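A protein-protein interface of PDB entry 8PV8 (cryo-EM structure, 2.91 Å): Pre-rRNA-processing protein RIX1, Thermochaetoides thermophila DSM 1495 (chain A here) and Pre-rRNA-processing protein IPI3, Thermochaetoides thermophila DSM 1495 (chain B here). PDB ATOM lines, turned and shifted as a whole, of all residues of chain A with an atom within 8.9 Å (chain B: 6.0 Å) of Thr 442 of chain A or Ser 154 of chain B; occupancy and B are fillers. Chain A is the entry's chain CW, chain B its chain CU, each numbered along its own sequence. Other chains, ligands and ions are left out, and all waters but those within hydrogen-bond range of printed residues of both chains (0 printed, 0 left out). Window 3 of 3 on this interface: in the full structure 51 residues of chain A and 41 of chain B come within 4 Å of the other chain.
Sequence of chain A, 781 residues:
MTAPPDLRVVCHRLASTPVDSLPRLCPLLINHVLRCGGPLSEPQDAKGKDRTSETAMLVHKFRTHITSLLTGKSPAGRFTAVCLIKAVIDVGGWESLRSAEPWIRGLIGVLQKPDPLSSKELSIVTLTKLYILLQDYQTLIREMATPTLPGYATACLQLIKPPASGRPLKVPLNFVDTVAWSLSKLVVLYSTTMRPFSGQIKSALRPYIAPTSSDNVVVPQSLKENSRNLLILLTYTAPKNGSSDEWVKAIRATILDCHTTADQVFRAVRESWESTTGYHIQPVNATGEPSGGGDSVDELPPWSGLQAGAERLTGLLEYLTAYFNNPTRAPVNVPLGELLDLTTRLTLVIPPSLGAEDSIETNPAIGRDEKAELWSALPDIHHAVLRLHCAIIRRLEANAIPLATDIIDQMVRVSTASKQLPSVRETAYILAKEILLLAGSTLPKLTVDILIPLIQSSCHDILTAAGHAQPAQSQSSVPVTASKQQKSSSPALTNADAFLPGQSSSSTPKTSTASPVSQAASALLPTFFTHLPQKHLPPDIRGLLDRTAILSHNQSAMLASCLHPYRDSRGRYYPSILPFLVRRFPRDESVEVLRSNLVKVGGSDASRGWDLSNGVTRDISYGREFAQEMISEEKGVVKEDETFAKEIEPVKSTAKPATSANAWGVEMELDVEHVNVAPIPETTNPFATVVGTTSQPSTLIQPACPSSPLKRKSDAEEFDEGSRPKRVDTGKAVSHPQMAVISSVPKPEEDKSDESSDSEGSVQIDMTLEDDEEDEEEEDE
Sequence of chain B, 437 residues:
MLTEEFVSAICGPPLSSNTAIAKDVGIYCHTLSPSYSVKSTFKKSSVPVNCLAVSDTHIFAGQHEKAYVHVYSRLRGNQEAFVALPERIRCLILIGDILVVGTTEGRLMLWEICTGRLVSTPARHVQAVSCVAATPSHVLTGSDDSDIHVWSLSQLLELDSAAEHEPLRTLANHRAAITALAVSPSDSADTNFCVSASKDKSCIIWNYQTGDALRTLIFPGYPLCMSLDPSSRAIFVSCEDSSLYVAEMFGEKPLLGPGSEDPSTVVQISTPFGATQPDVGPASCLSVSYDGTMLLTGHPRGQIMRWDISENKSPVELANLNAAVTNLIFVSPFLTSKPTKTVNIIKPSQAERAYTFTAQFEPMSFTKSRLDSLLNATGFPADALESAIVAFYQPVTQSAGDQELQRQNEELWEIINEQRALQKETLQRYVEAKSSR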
ATOM      1  N   ALA A 398      21.645  16.897 -21.634  1.00  0.00           N
ATOM      2  CA  ALA A 398      20.239  16.507 -21.629  1.00  0.00           C
ATOM      3  C   ALA A 398      19.953  15.289 -20.761  1.00  0.00           C
ATOM      4  O   ALA A 398      18.780  14.957 -20.562  1.00  0.00           O
ATOM      5  CB  ALA A 398      19.767  16.239 -23.059  1.00  0.00           C
ATOM      6  N   ALA A 400      20.744  15.214 -17.627  1.00  0.00           N
ATOM      7  CA  ALA A 400      20.450  15.755 -16.309  1.00  0.00           C
ATOM      8  C   ALA A 400      19.021  16.264 -16.192  1.00  0.00           C
ATOM      9  O   ALA A 400      18.647  16.775 -15.130  1.00  0.00           O
ATOM     10  CB  ALA A 400      21.429  16.883 -15.962  1.00  0.00           C
ATOM     11  N   ILE A 401      18.230  16.163 -17.265  1.00  0.00           N
ATOM     12  CA  ILE A 401      16.784  16.394 -17.151  1.00  0.00           C
ATOM     13  C   ILE A 401      16.114  15.499 -16.113  1.00  0.00           C
ATOM     14  O   ILE A 401      15.235  15.997 -15.391  1.00  0.00           O
ATOM     15  CB  ILE A 401      16.129  16.318 -18.538  1.00  0.00           C
ATOM     16  CG1 ILE A 401      16.801  17.307 -19.493  1.00  0.00           C
ATOM     17  CG2 ILE A 401      14.638  16.617 -18.464  1.00  0.00           C
ATOM     18  CD1 ILE A 401      16.211  17.315 -20.887  1.00  0.00           C
ATOM     19  N   PRO A 402      16.439  14.195 -15.973  1.00  0.00           N
ATOM     20  CA  PRO A 402      15.883  13.448 -14.825  1.00  0.00           C
ATOM     21  C   PRO A 402      16.263  14.025 -13.475  1.00  0.00           C
ATOM     22  O   PRO A 402      15.466  13.953 -12.530  1.00  0.00           O
ATOM     23  CB  PRO A 402      16.473  12.043 -14.998  1.00  0.00           C
ATOM     24  CG  PRO A 402      16.721  11.913 -16.410  1.00  0.00           C
ATOM     25  CD  PRO A 402      17.162  13.267 -16.871  1.00  0.00           C
ATOM     26  N   LEU A 403      17.454  14.602 -13.357  1.00  0.00           N
ATOM     27  CA  LEU A 403      17.933  15.163 -12.106  1.00  0.00           C
ATOM     28  C   LEU A 403      17.462  16.593 -11.881  1.00  0.00           C
ATOM     29  O   LEU A 403      17.728  17.150 -10.813  1.00  0.00           O
ATOM     30  CB  LEU A 403      19.467  15.131 -12.073  1.00  0.00           C
ATOM     31  CG  LEU A 403      20.167  13.788 -11.852  1.00  0.00           C
ATOM     32  CD1 LEU A 403      21.614  13.994 -11.427  1.00  0.00           C
ATOM     33  CD2 LEU A 403      19.424  12.935 -10.854  1.00  0.00           C
ATOM     34  N   ALA A 404      16.753  17.184 -12.846  1.00  0.00           N
ATOM     35  CA  ALA A 404      16.593  18.636 -12.882  1.00  0.00           C
ATOM     36  C   ALA A 404      15.661  19.148 -11.791  1.00  0.00           C
ATOM     37  O   ALA A 404      15.828  20.273 -11.307  1.00  0.00           O
ATOM     38  CB  ALA A 404      16.089  19.071 -14.258  1.00  0.00           C
ATOM     39  N   THR A 405      14.668  18.345 -11.398  1.00  0.00           N
ATOM     40  CA  THR A 405      13.636  18.825 -10.479  1.00  0.00           C
ATOM     41  C   THR A 405      14.196  19.098  -9.085  1.00  0.00           C
ATOM     42  O   THR A 405      13.839  20.098  -8.450  1.00  0.00           O
ATOM     43  CB  THR A 405      12.491  17.815 -10.408  1.00  0.00           C
ATOM     44  OG1 THR A 405      12.073  17.475 -11.736  1.00  0.00           O
ATOM     45  CG2 THR A 405      11.307  18.395  -9.649  1.00  0.00           C
ATOM     46  N   ILE A 408      16.495  22.348  -8.747  1.00  0.00           N
ATOM     47  CA  ILE A 408      15.757  23.604  -8.605  1.00  0.00           C
ATOM     48  C   ILE A 408      15.430  23.866  -7.141  1.00  0.00           C
ATOM     49  O   ILE A 408      15.622  24.978  -6.632  1.00  0.00           O
ATOM     50  CB  ILE A 408      14.476  23.577  -9.460  1.00  0.00           C
ATOM     51  CG1 ILE A 408      14.810  23.337 -10.930  1.00  0.00           C
ATOM     52  CG2 ILE A 408      13.705  24.877  -9.299  1.00  0.00           C
ATOM     53  CD1 ILE A 408      13.623  23.437 -11.858  1.00  0.00           C
ATOM     54  N   ILE A 435      20.066  25.115 -15.710  1.00  0.00           N
ATOM     55  CA  ILE A 435      18.907  24.239 -15.555  1.00  0.00           C
ATOM     56  C   ILE A 435      17.713  24.770 -16.343  1.00  0.00           C
ATOM     57  O   ILE A 435      16.862  23.994 -16.794  1.00  0.00           O
ATOM     58  CB  ILE A 435      18.568  24.030 -14.068  1.00  0.00           C
ATOM     59  CG1 ILE A 435      18.193  25.348 -13.396  1.00  0.00           C
ATOM     60  CG2 ILE A 435      19.731  23.371 -13.344  1.00  0.00           C
ATOM     61  CD1 ILE A 435      17.735  25.190 -11.986  1.00  0.00           C
ATOM     62  N   LEU A 436      17.627  26.091 -16.535  1.00  0.00           N
ATOM     63  CA  LEU A 436      16.552  26.630 -17.356  1.00  0.00           C
ATOM     64  C   LEU A 436      16.795  26.408 -18.841  1.00  0.00           C
ATOM     65  O   LEU A 436      15.833  26.169 -19.578  1.00  0.00           O
ATOM     66  CB  LEU A 436      16.350  28.118 -17.071  1.00  0.00           C
ATOM     67  CG  LEU A 436      15.657  28.486 -15.755  1.00  0.00           C
ATOM     68  CD1 LEU A 436      15.396  29.981 -15.684  1.00  0.00           C
ATOM     69  CD2 LEU A 436      14.366  27.708 -15.590  1.00  0.00           C
ATOM     70  N   LEU A 438      18.253  23.764 -19.908  1.00  0.00           N
ATOM     71  CA  LEU A 438      17.923  22.360 -20.130  1.00  0.00           C
ATOM     72  C   LEU A 438      16.420  22.112 -20.076  1.00  0.00           C
ATOM     73  O   LEU A 438      15.820  21.724 -21.083  1.00  0.00           O
ATOM     74  CB  LEU A 438      18.628  21.458 -19.120  1.00  0.00           C
ATOM     75  CG  LEU A 438      20.127  21.285 -19.329  1.00  0.00           C
ATOM     76  CD1 LEU A 438      20.686  20.433 -18.222  1.00  0.00           C
ATOM     77  CD2 LEU A 438      20.408  20.663 -20.684  1.00  0.00           C
ATOM     78  N   ALA A 439      15.799  22.327 -18.918  1.00  0.00           N
ATOM     79  CA  ALA A 439      14.364  22.105 -18.738  1.00  0.00           C
ATOM     80  C   ALA A 439      13.768  23.316 -18.026  1.00  0.00           C
ATOM     81  O   ALA A 439      13.628  23.327 -16.802  1.00  0.00           O
ATOM     82  CB  ALA A 439      14.108  20.814 -17.963  1.00  0.00           C
ATOM     83  N   GLY A 440      13.414  24.337 -18.801  1.00  0.00           N
ATOM     84  CA  GLY A 440      12.778  25.512 -18.241  1.00  0.00           C
ATOM     85  C   GLY A 440      11.459  25.862 -18.898  1.00  0.00           C
ATOM     86  O   GLY A 440      10.607  26.515 -18.288  1.00  0.00           O
ATOM     87  N   SER A 441      11.278  25.429 -20.146  1.00  0.00           N
ATOM     88  CA  SER A 441      10.112  25.822 -20.928  1.00  0.00           C
ATOM     89  C   SER A 441       8.835  25.114 -20.498  1.00  0.00           C
ATOM     90  O   SER A 441       7.748  25.557 -20.883  1.00  0.00           O
ATOM     91  CB  SER A 441      10.370  25.561 -22.414  1.00  0.00           C
ATOM     92  OG  SER A 441      10.781  24.224 -22.633  1.00  0.00           O
ATOM     93  N   THR A 442       8.931  24.036 -19.717  1.00  0.00           N
ATOM     94  CA  THR A 442       7.751  23.302 -19.275  1.00  0.00           C
ATOM     95  C   THR A 442       7.701  23.166 -17.759  1.00  0.00           C
ATOM     96  O   THR A 442       7.150  22.184 -17.249  1.00  0.00           O
ATOM     97  CB  THR A 442       7.693  21.918 -19.924  1.00  0.00           C
ATOM     98  OG1 THR A 442       8.992  21.313 -19.883  1.00  0.00           O
ATOM     99  CG2 THR A 442       7.237  22.030 -21.364  1.00  0.00           C
ATOM    100  N   LEU A 443       8.270  24.119 -17.031  1.00  0.00           N
ATOM    101  CA  LEU A 443       8.196  24.082 -15.581  1.00  0.00           C
ATOM    102  C   LEU A 443       6.774  24.404 -15.127  1.00  0.00           C
ATOM    103  O   LEU A 443       6.108  25.254 -15.729  1.00  0.00           O
ATOM    104  CB  LEU A 443       9.183  25.072 -14.966  1.00  0.00           C
ATOM    105  CG  LEU A 443      10.646  24.633 -14.989  1.00  0.00           C
ATOM    106  CD1 LEU A 443      11.520  25.661 -14.296  1.00  0.00           C
ATOM    107  CD2 LEU A 443      10.805  23.264 -14.345  1.00  0.00           C
ATOM    108  N   PRO A 444       6.276  23.747 -14.084  1.00  0.00           N
ATOM    109  CA  PRO A 444       4.918  24.027 -13.617  1.00  0.00           C
ATOM    110  C   PRO A 444       4.827  25.348 -12.869  1.00  0.00           C
ATOM    111  O   PRO A 444       5.835  25.987 -12.546  1.00  0.00           O
ATOM    112  CB  PRO A 444       4.613  22.845 -12.691  1.00  0.00           C
ATOM    113  CG  PRO A 444       5.942  22.400 -12.206  1.00  0.00           C
ATOM    114  CD  PRO A 444       6.909  22.651 -13.329  1.00  0.00           C
ATOM    115  N   LYS A 445       3.582  25.743 -12.600  1.00  0.00           N
ATOM    116  CA  LYS A 445       3.248  27.019 -11.976  1.00  0.00           C
ATOM    117  C   LYS A 445       3.883  27.155 -10.598  1.00  0.00           C
ATOM    118  O   LYS A 445       4.329  28.244 -10.227  1.00  0.00           O
ATOM    119  CB  LYS A 445       1.726  27.167 -11.884  1.00  0.00           C
ATOM    120  CG  LYS A 445       1.245  28.404 -11.144  1.00  0.00           C
ATOM    121  CD  LYS A 445       1.218  29.619 -12.053  1.00  0.00           C
ATOM    122  CE  LYS A 445       0.660  30.833 -11.329  1.00  0.00           C
ATOM    123  NZ  LYS A 445       0.527  32.009 -12.234  1.00  0.00           N
ATOM    124  N   THR A 447       6.751  25.768  -9.595  1.00  0.00           N
ATOM    125  CA  THR A 447       8.174  26.034  -9.786  1.00  0.00           C
ATOM    126  C   THR A 447       8.411  27.465 -10.258  1.00  0.00           C
ATOM    127  O   THR A 447       9.346  28.132  -9.792  1.00  0.00           O
ATOM    128  CB  THR A 447       8.762  25.030 -10.775  1.00  0.00           C
ATOM    129  OG1 THR A 447       8.410  23.701 -10.373  1.00  0.00           O
ATOM    130  CG2 THR A 447      10.274  25.145 -10.813  1.00  0.00           C
ATOM    131  N   VAL A 448       7.566  27.955 -11.171  1.00  0.00           N
ATOM    132  CA  VAL A 448       7.663  29.346 -11.606  1.00  0.00           C
ATOM    133  C   VAL A 448       7.438  30.312 -10.448  1.00  0.00           C
ATOM    134  O   VAL A 448       8.145  31.321 -10.340  1.00  0.00           O
ATOM    135  CB  VAL A 448       6.676  29.611 -12.761  1.00  0.00           C
ATOM    136  CG1 VAL A 448       6.751  31.055 -13.219  1.00  0.00           C
ATOM    137  CG2 VAL A 448       6.981  28.693 -13.930  1.00  0.00           C
ATOM    138  N   THR A 530      13.388  33.588 -22.630  1.00  0.00           N
ATOM    139  CA  THR A 530      13.487  32.506 -23.610  1.00  0.00           C
ATOM    140  C   THR A 530      13.016  31.174 -23.041  1.00  0.00           C
ATOM    141  O   THR A 530      12.260  30.448 -23.697  1.00  0.00           O
ATOM    142  CB  THR A 530      14.920  32.372 -24.125  1.00  0.00           C
ATOM    143  OG1 THR A 530      15.817  32.198 -23.023  1.00  0.00           O
ATOM    144  CG2 THR A 530      15.325  33.596 -24.919  1.00  0.00           C
ATOM    145  N   HIS A 531      13.444  30.830 -21.827  1.00  0.00           N
ATOM    146  CA  HIS A 531      13.226  29.499 -21.281  1.00  0.00           C
ATOM    147  C   HIS A 531      12.431  29.510 -19.983  1.00  0.00           C
ATOM    148  O   HIS A 531      12.718  28.711 -19.086  1.00  0.00           O
ATOM    149  CB  HIS A 531      14.568  28.799 -21.068  1.00  0.00           C
ATOM    150  CG  HIS A 531      15.216  28.345 -22.338  1.00  0.00           C
ATOM    151  ND1 HIS A 531      16.071  29.144 -23.065  1.00  0.00           N
ATOM    152  CD2 HIS A 531      15.131  27.173 -23.012  1.00  0.00           C
ATOM    153  CE1 HIS A 531      16.486  28.485 -24.131  1.00  0.00           C
ATOM    154  NE2 HIS A 531      15.932  27.287 -24.122  1.00  0.00           N
ATOM    155  N   LEU A 532      11.455  30.401 -19.852  1.00  0.00           N
ATOM    156  CA  LEU A 532      10.532  30.391 -18.737  1.00  0.00           C
ATOM    157  C   LEU A 532       9.124  30.628 -19.266  1.00  0.00           C
ATOM    158  O   LEU A 532       8.947  31.447 -20.180  1.00  0.00           O
ATOM    159  CB  LEU A 532      10.900  31.468 -17.705  1.00  0.00           C
ATOM    160  CG  LEU A 532      10.574  31.179 -16.238  1.00  0.00           C
ATOM    161  CD1 LEU A 532      11.153  29.841 -15.815  1.00  0.00           C
ATOM    162  CD2 LEU A 532      11.093  32.293 -15.345  1.00  0.00           C
ATOM    163  N   PRO A 533       8.112  29.929 -18.753  1.00  0.00           N
ATOM    164  CA  PRO A 533       6.750  30.120 -19.268  1.00  0.00           C
ATOM    165  C   PRO A 533       6.208  31.496 -18.910  1.00  0.00           C
ATOM    166  O   PRO A 533       6.104  31.858 -17.735  1.00  0.00           O
ATOM    167  CB  PRO A 533       5.952  29.001 -18.589  1.00  0.00           C
ATOM    168  CG  PRO A 533       6.971  27.999 -18.169  1.00  0.00           C
ATOM    169  CD  PRO A 533       8.196  28.786 -17.831  1.00  0.00           C
ATOM    170  N   GLN A 534       5.865  32.266 -19.944  1.00  0.00           N
ATOM    171  CA  GLN A 534       5.390  33.628 -19.731  1.00  0.00           C
ATOM    172  C   GLN A 534       3.976  33.641 -19.165  1.00  0.00           C
ATOM    173  O   GLN A 534       3.582  34.600 -18.491  1.00  0.00           O
ATOM    174  CB  GLN A 534       5.448  34.413 -21.041  1.00  0.00           C
ATOM    175  CG  GLN A 534       6.846  34.543 -21.622  1.00  0.00           C
ATOM    176  CD  GLN A 534       7.866  34.986 -20.596  1.00  0.00           C
ATOM    177  OE1 GLN A 534       7.724  36.042 -19.980  1.00  0.00           O
ATOM    178  NE2 GLN A 534       8.902  34.181 -20.405  1.00  0.00           N
ATOM    179  N   LYS A 535       3.196  32.591 -19.433  1.00  0.00           N
ATOM    180  CA  LYS A 535       1.831  32.534 -18.924  1.00  0.00           C
ATOM    181  C   LYS A 535       1.808  32.344 -17.413  1.00  0.00           C
ATOM    182  O   LYS A 535       0.882  32.804 -16.734  1.00  0.00           O
ATOM    183  CB  LYS A 535       1.060  31.411 -19.618  1.00  0.00           C
ATOM    184  CG  LYS A 535       1.853  30.127 -19.787  1.00  0.00           C
ATOM    185  CD  LYS A 535       1.036  29.065 -20.502  1.00  0.00           C
ATOM    186  CE  LYS A 535       1.797  27.754 -20.594  1.00  0.00           C
ATOM    187  NZ  LYS A 535       1.012  26.707 -21.303  1.00  0.00           N
ATOM    188  N   HIS A 536       2.822  31.669 -16.865  1.00  0.00           N
ATOM    189  CA  HIS A 536       2.855  31.430 -15.428  1.00  0.00           C
ATOM    190  C   HIS A 536       3.437  32.615 -14.667  1.00  0.00           C
ATOM    191  O   HIS A 536       3.327  32.674 -13.438  1.00  0.00           O
ATOM    192  CB  HIS A 536       3.654  30.163 -15.129  1.00  0.00           C
ATOM    193  CG  HIS A 536       3.072  28.926 -15.739  1.00  0.00           C
ATOM    194  ND1 HIS A 536       1.759  28.845 -16.149  1.00  0.00           N
ATOM    195  CD2 HIS A 536       3.627  27.722 -16.015  1.00  0.00           C
ATOM    196  CE1 HIS A 536       1.529  27.644 -16.647  1.00  0.00           C
ATOM    197  NE2 HIS A 536       2.646  26.943 -16.577  1.00  0.00           N
ATOM    198  N   SER B 137      12.080  19.365 -25.268  1.00  0.00           N
ATOM    199  CA  SER B 137      11.117  19.665 -24.217  1.00  0.00           C
ATOM    200  C   SER B 137       9.742  19.049 -24.429  1.00  0.00           C
ATOM    201  O   SER B 137       8.908  19.154 -23.522  1.00  0.00           O
ATOM    202  CB  SER B 137      10.956  21.182 -24.055  1.00  0.00           C
ATOM    203  OG  SER B 137      10.553  21.783 -25.273  1.00  0.00           O
ATOM    204  N   HIS B 138       9.452  18.413 -25.566  1.00  0.00           N
ATOM    205  CA  HIS B 138       8.103  17.934 -25.838  1.00  0.00           C
ATOM    206  C   HIS B 138       8.123  16.622 -26.612  1.00  0.00           C
ATOM    207  O   HIS B 138       9.062  16.316 -27.346  1.00  0.00           O
ATOM    208  CB  HIS B 138       7.286  18.966 -26.627  1.00  0.00           C
ATOM    209  CG  HIS B 138       6.865  20.153 -25.819  1.00  0.00           C
ATOM    210  ND1 HIS B 138       7.687  21.238 -25.608  1.00  0.00           N
ATOM    211  CD2 HIS B 138       5.708  20.426 -25.172  1.00  0.00           C
ATOM    212  CE1 HIS B 138       7.054  22.130 -24.868  1.00  0.00           C
ATOM    213  NE2 HIS B 138       5.851  21.661 -24.588  1.00  0.00           N
ATOM    214  N   SER B 152       5.214  16.596 -21.841  1.00  0.00           N
ATOM    215  CA  SER B 152       6.445  17.253 -21.424  1.00  0.00           C
ATOM    216  C   SER B 152       7.453  16.183 -21.029  1.00  0.00           C
ATOM    217  O   SER B 152       7.119  15.266 -20.272  1.00  0.00           O
ATOM    218  CB  SER B 152       6.190  18.209 -20.260  1.00  0.00           C
ATOM    219  OG  SER B 152       7.410  18.604 -19.657  1.00  0.00           O
ATOM    220  N   LEU B 153       8.676  16.292 -21.556  1.00  0.00           N
ATOM    221  CA  LEU B 153       9.720  15.327 -21.217  1.00  0.00           C
ATOM    222  C   LEU B 153      10.107  15.409 -19.748  1.00  0.00           C
ATOM    223  O   LEU B 153      10.341  14.380 -19.103  1.00  0.00           O
ATOM    224  CB  LEU B 153      10.947  15.540 -22.097  1.00  0.00           C
ATOM    225  CG  LEU B 153      10.946  14.814 -23.438  1.00  0.00           C
ATOM    226  CD1 LEU B 153      12.105  15.292 -24.285  1.00  0.00           C
ATOM    227  CD2 LEU B 153      11.027  13.318 -23.210  1.00  0.00           C
ATOM    228  N   SER B 154      10.193  16.625 -19.201  1.00  0.00           N
ATOM    229  CA  SER B 154      10.547  16.780 -17.794  1.00  0.00           C
ATOM    230  C   SER B 154       9.468  16.222 -16.872  1.00  0.00           C
ATOM    231  O   SER B 154       9.766  15.849 -15.732  1.00  0.00           O
ATOM    232  CB  SER B 154      10.797  18.252 -17.475  1.00  0.00           C
ATOM    233  OG  SER B 154       9.641  19.024 -17.742  1.00  0.00           O
ATOM    234  N   GLN B 155       8.221  16.162 -17.338  1.00  0.00           N
ATOM    235  CA  GLN B 155       7.145  15.539 -16.578  1.00  0.00           C
ATOM    236  C   GLN B 155       7.100  14.031 -16.780  1.00  0.00           C
ATOM    237  O   GLN B 155       6.747  13.299 -15.850  1.00  0.00           O
ATOM    238  CB  GLN B 155       5.797  16.170 -16.959  1.00  0.00           C
ATOM    239  CG  GLN B 155       4.588  15.670 -16.164  1.00  0.00           C
ATOM    240  CD  GLN B 155       3.305  16.378 -16.555  1.00  0.00           C
ATOM    241  OE1 GLN B 155       3.302  17.225 -17.446  1.00  0.00           O
ATOM    242  NE2 GLN B 155       2.203  16.018 -15.905  1.00  0.00           N
ATOM    243  N   LEU B 156       7.443  13.552 -17.980  1.00  0.00           N
ATOM    244  CA  LEU B 156       7.462  12.115 -18.236  1.00  0.00           C
ATOM    245  C   LEU B 156       8.590  11.428 -17.480  1.00  0.00           C
ATOM    246  O   LEU B 156       8.377  10.401 -16.826  1.00  0.00           O
ATOM    247  CB  LEU B 156       7.599  11.847 -19.735  1.00  0.00           C
ATOM    248  CG  LEU B 156       6.367  12.067 -20.615  1.00  0.00           C
ATOM    249  CD1 LEU B 156       6.670  11.735 -22.072  1.00  0.00           C
ATOM    250  CD2 LEU B 156       5.197  11.249 -20.100  1.00  0.00           C
ATOM    251  N   LEU B 157       9.795  11.978 -17.555  1.00  0.00           N
ATOM    252  CA  LEU B 157      10.977  11.357 -16.976  1.00  0.00           C
ATOM    253  C   LEU B 157      11.502  12.200 -15.816  1.00  0.00           C
ATOM    254  O   LEU B 157      11.922  13.346 -16.001  1.00  0.00           O
ATOM    255  CB  LEU B 157      12.011  11.096 -18.080  1.00  0.00           C
ATOM    256  CG  LEU B 157      12.686  12.132 -18.990  1.00  0.00           C
ATOM    257  CD1 LEU B 157      13.882  12.823 -18.408  1.00  0.00           C
ATOM    258  CD2 LEU B 157      13.072  11.472 -20.299  1.00  0.00           C
ATOM    259  N   GLU B 158      11.378  11.654 -14.607  1.00  0.00           N
ATOM    260  CA  GLU B 158      11.972  12.210 -13.399  1.00  0.00           C
ATOM    261  C   GLU B 158      12.255  11.070 -12.433  1.00  0.00           C
ATOM    262  O   GLU B 158      11.785   9.946 -12.631  1.00  0.00           O
ATOM    263  CB  GLU B 158      11.068  13.252 -12.729  1.00  0.00           C
ATOM    264  CG  GLU B 158       9.807  12.675 -12.110  1.00  0.00           C
ATOM    265  CD  GLU B 158       8.669  12.526 -13.106  1.00  0.00           C
ATOM    266  OE1 GLU B 158       8.919  12.583 -14.323  1.00  0.00           O
ATOM    267  OE2 GLU B 158       7.512  12.372 -12.672  1.00  0.00           O
ATOM    268  N   LEU B 168      -0.277  17.149 -21.677  1.00  0.00           N
ATOM    269  CA  LEU B 168      -0.612  18.549 -21.437  1.00  0.00           C
ATOM    270  C   LEU B 168      -1.800  18.990 -22.283  1.00  0.00           C
ATOM    271  O   LEU B 168      -2.697  19.684 -21.791  1.00  0.00           O
ATOM    272  CB  LEU B 168       0.602  19.433 -21.721  1.00  0.00           C
ATOM    273  CG  LEU B 168       1.837  19.209 -20.850  1.00  0.00           C
ATOM    274  CD1 LEU B 168       2.994  20.070 -21.329  1.00  0.00           C
ATOM    275  CD2 LEU B 168       1.521  19.495 -19.391  1.00  0.00           C
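Of the printed residues of chain B, Thr 442 of chain A touches Ser 137 (3.96 Å), His 138 (3.5 Å), Ser 152 (3.1 Å) and Ser 154 (3.2 Å). Of the printed residues of chain A, His 138 of chain B touches Thr 442 (3.5 Å). Of the printed residues of chain A, Ser 152 of chain B touches Thr 442. Of the printed residues of chain A, Leu 157 of chain B touches Ile 401 (3.9 Å) and Pro 402 (3.6 Å). Leu 168 of chain B touches none of the printed residues of chain A. The nearest residue of chain B that does not touch Thr 442 of chain A is Leu 168 of chain B (4.7 Å). The nearest residue of chain A that does not touch Ser 154 of chain B is Ile 401 of chain A (4.1 Å). The nearest printed residue of chain A that does not touch Ser 137 of chain B is Leu 438 of chain A (5.7 Å).
CG2 of Ile 401 of chain A touches CD1 of Leu 157 of chain B, at 3.9 Å. Pro 402 of chain A touches Leu 157 of chain B (CG to CD1, 3.6 Å). CB of Ser 137 of chain B touches OG of Ser 441 of chain A, at 3.4 Å. Thr 442 of chain A touches Ser 137 of chain B. Thr 442 of chain A touches His 138 of chain B (CG2 to CE1, 3.5 Å).
Printed residues of chain B that touch a printed residue of chain A: Ser 137, His 138, Ser 152, Ser 154 and Leu 157. Hydrophobic or aromatic side chains of chain B that line the printed part of chain A: His 138 and Leu 157. Along chain B the printed residues that touch a printed residue of chain A span positions 137 to 157. Printed residues of chain A that touch a printed residue of chain B: Ile 401, Pro 402, Ser 441 and Thr 442. Among the printed residues, 7 pairs touch across the chains.
The side-chain hydroxyl of Ser 152 of chain B lies within hydrogen-bond range of the backbone NH of Gln 155 of chain B. OG of Ser 152 of chain B is in hydrogen-bond range of OG of Ser 154 of chain B. O of Ser 137 of chain B lies within hydrogen-bond range of N of Leu 153 of chain B (3.5 Å). The side-chain hydroxyl (OG) of Ser 137 of chain B lies within hydrogen-bond range of a ring nitrogen (ND1) of His 138 of chain B (2.9 Å).
The side-chain hydroxyl (OG1) of Thr 442 of chain A lies within hydrogen-bond range of the side-chain hydroxyl (OG) of Ser 154 of chain B (3.2 Å). OG of Ser 152 of chain B sits at hydrogen-bond distance from OG1 of Thr 442 of chain A.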
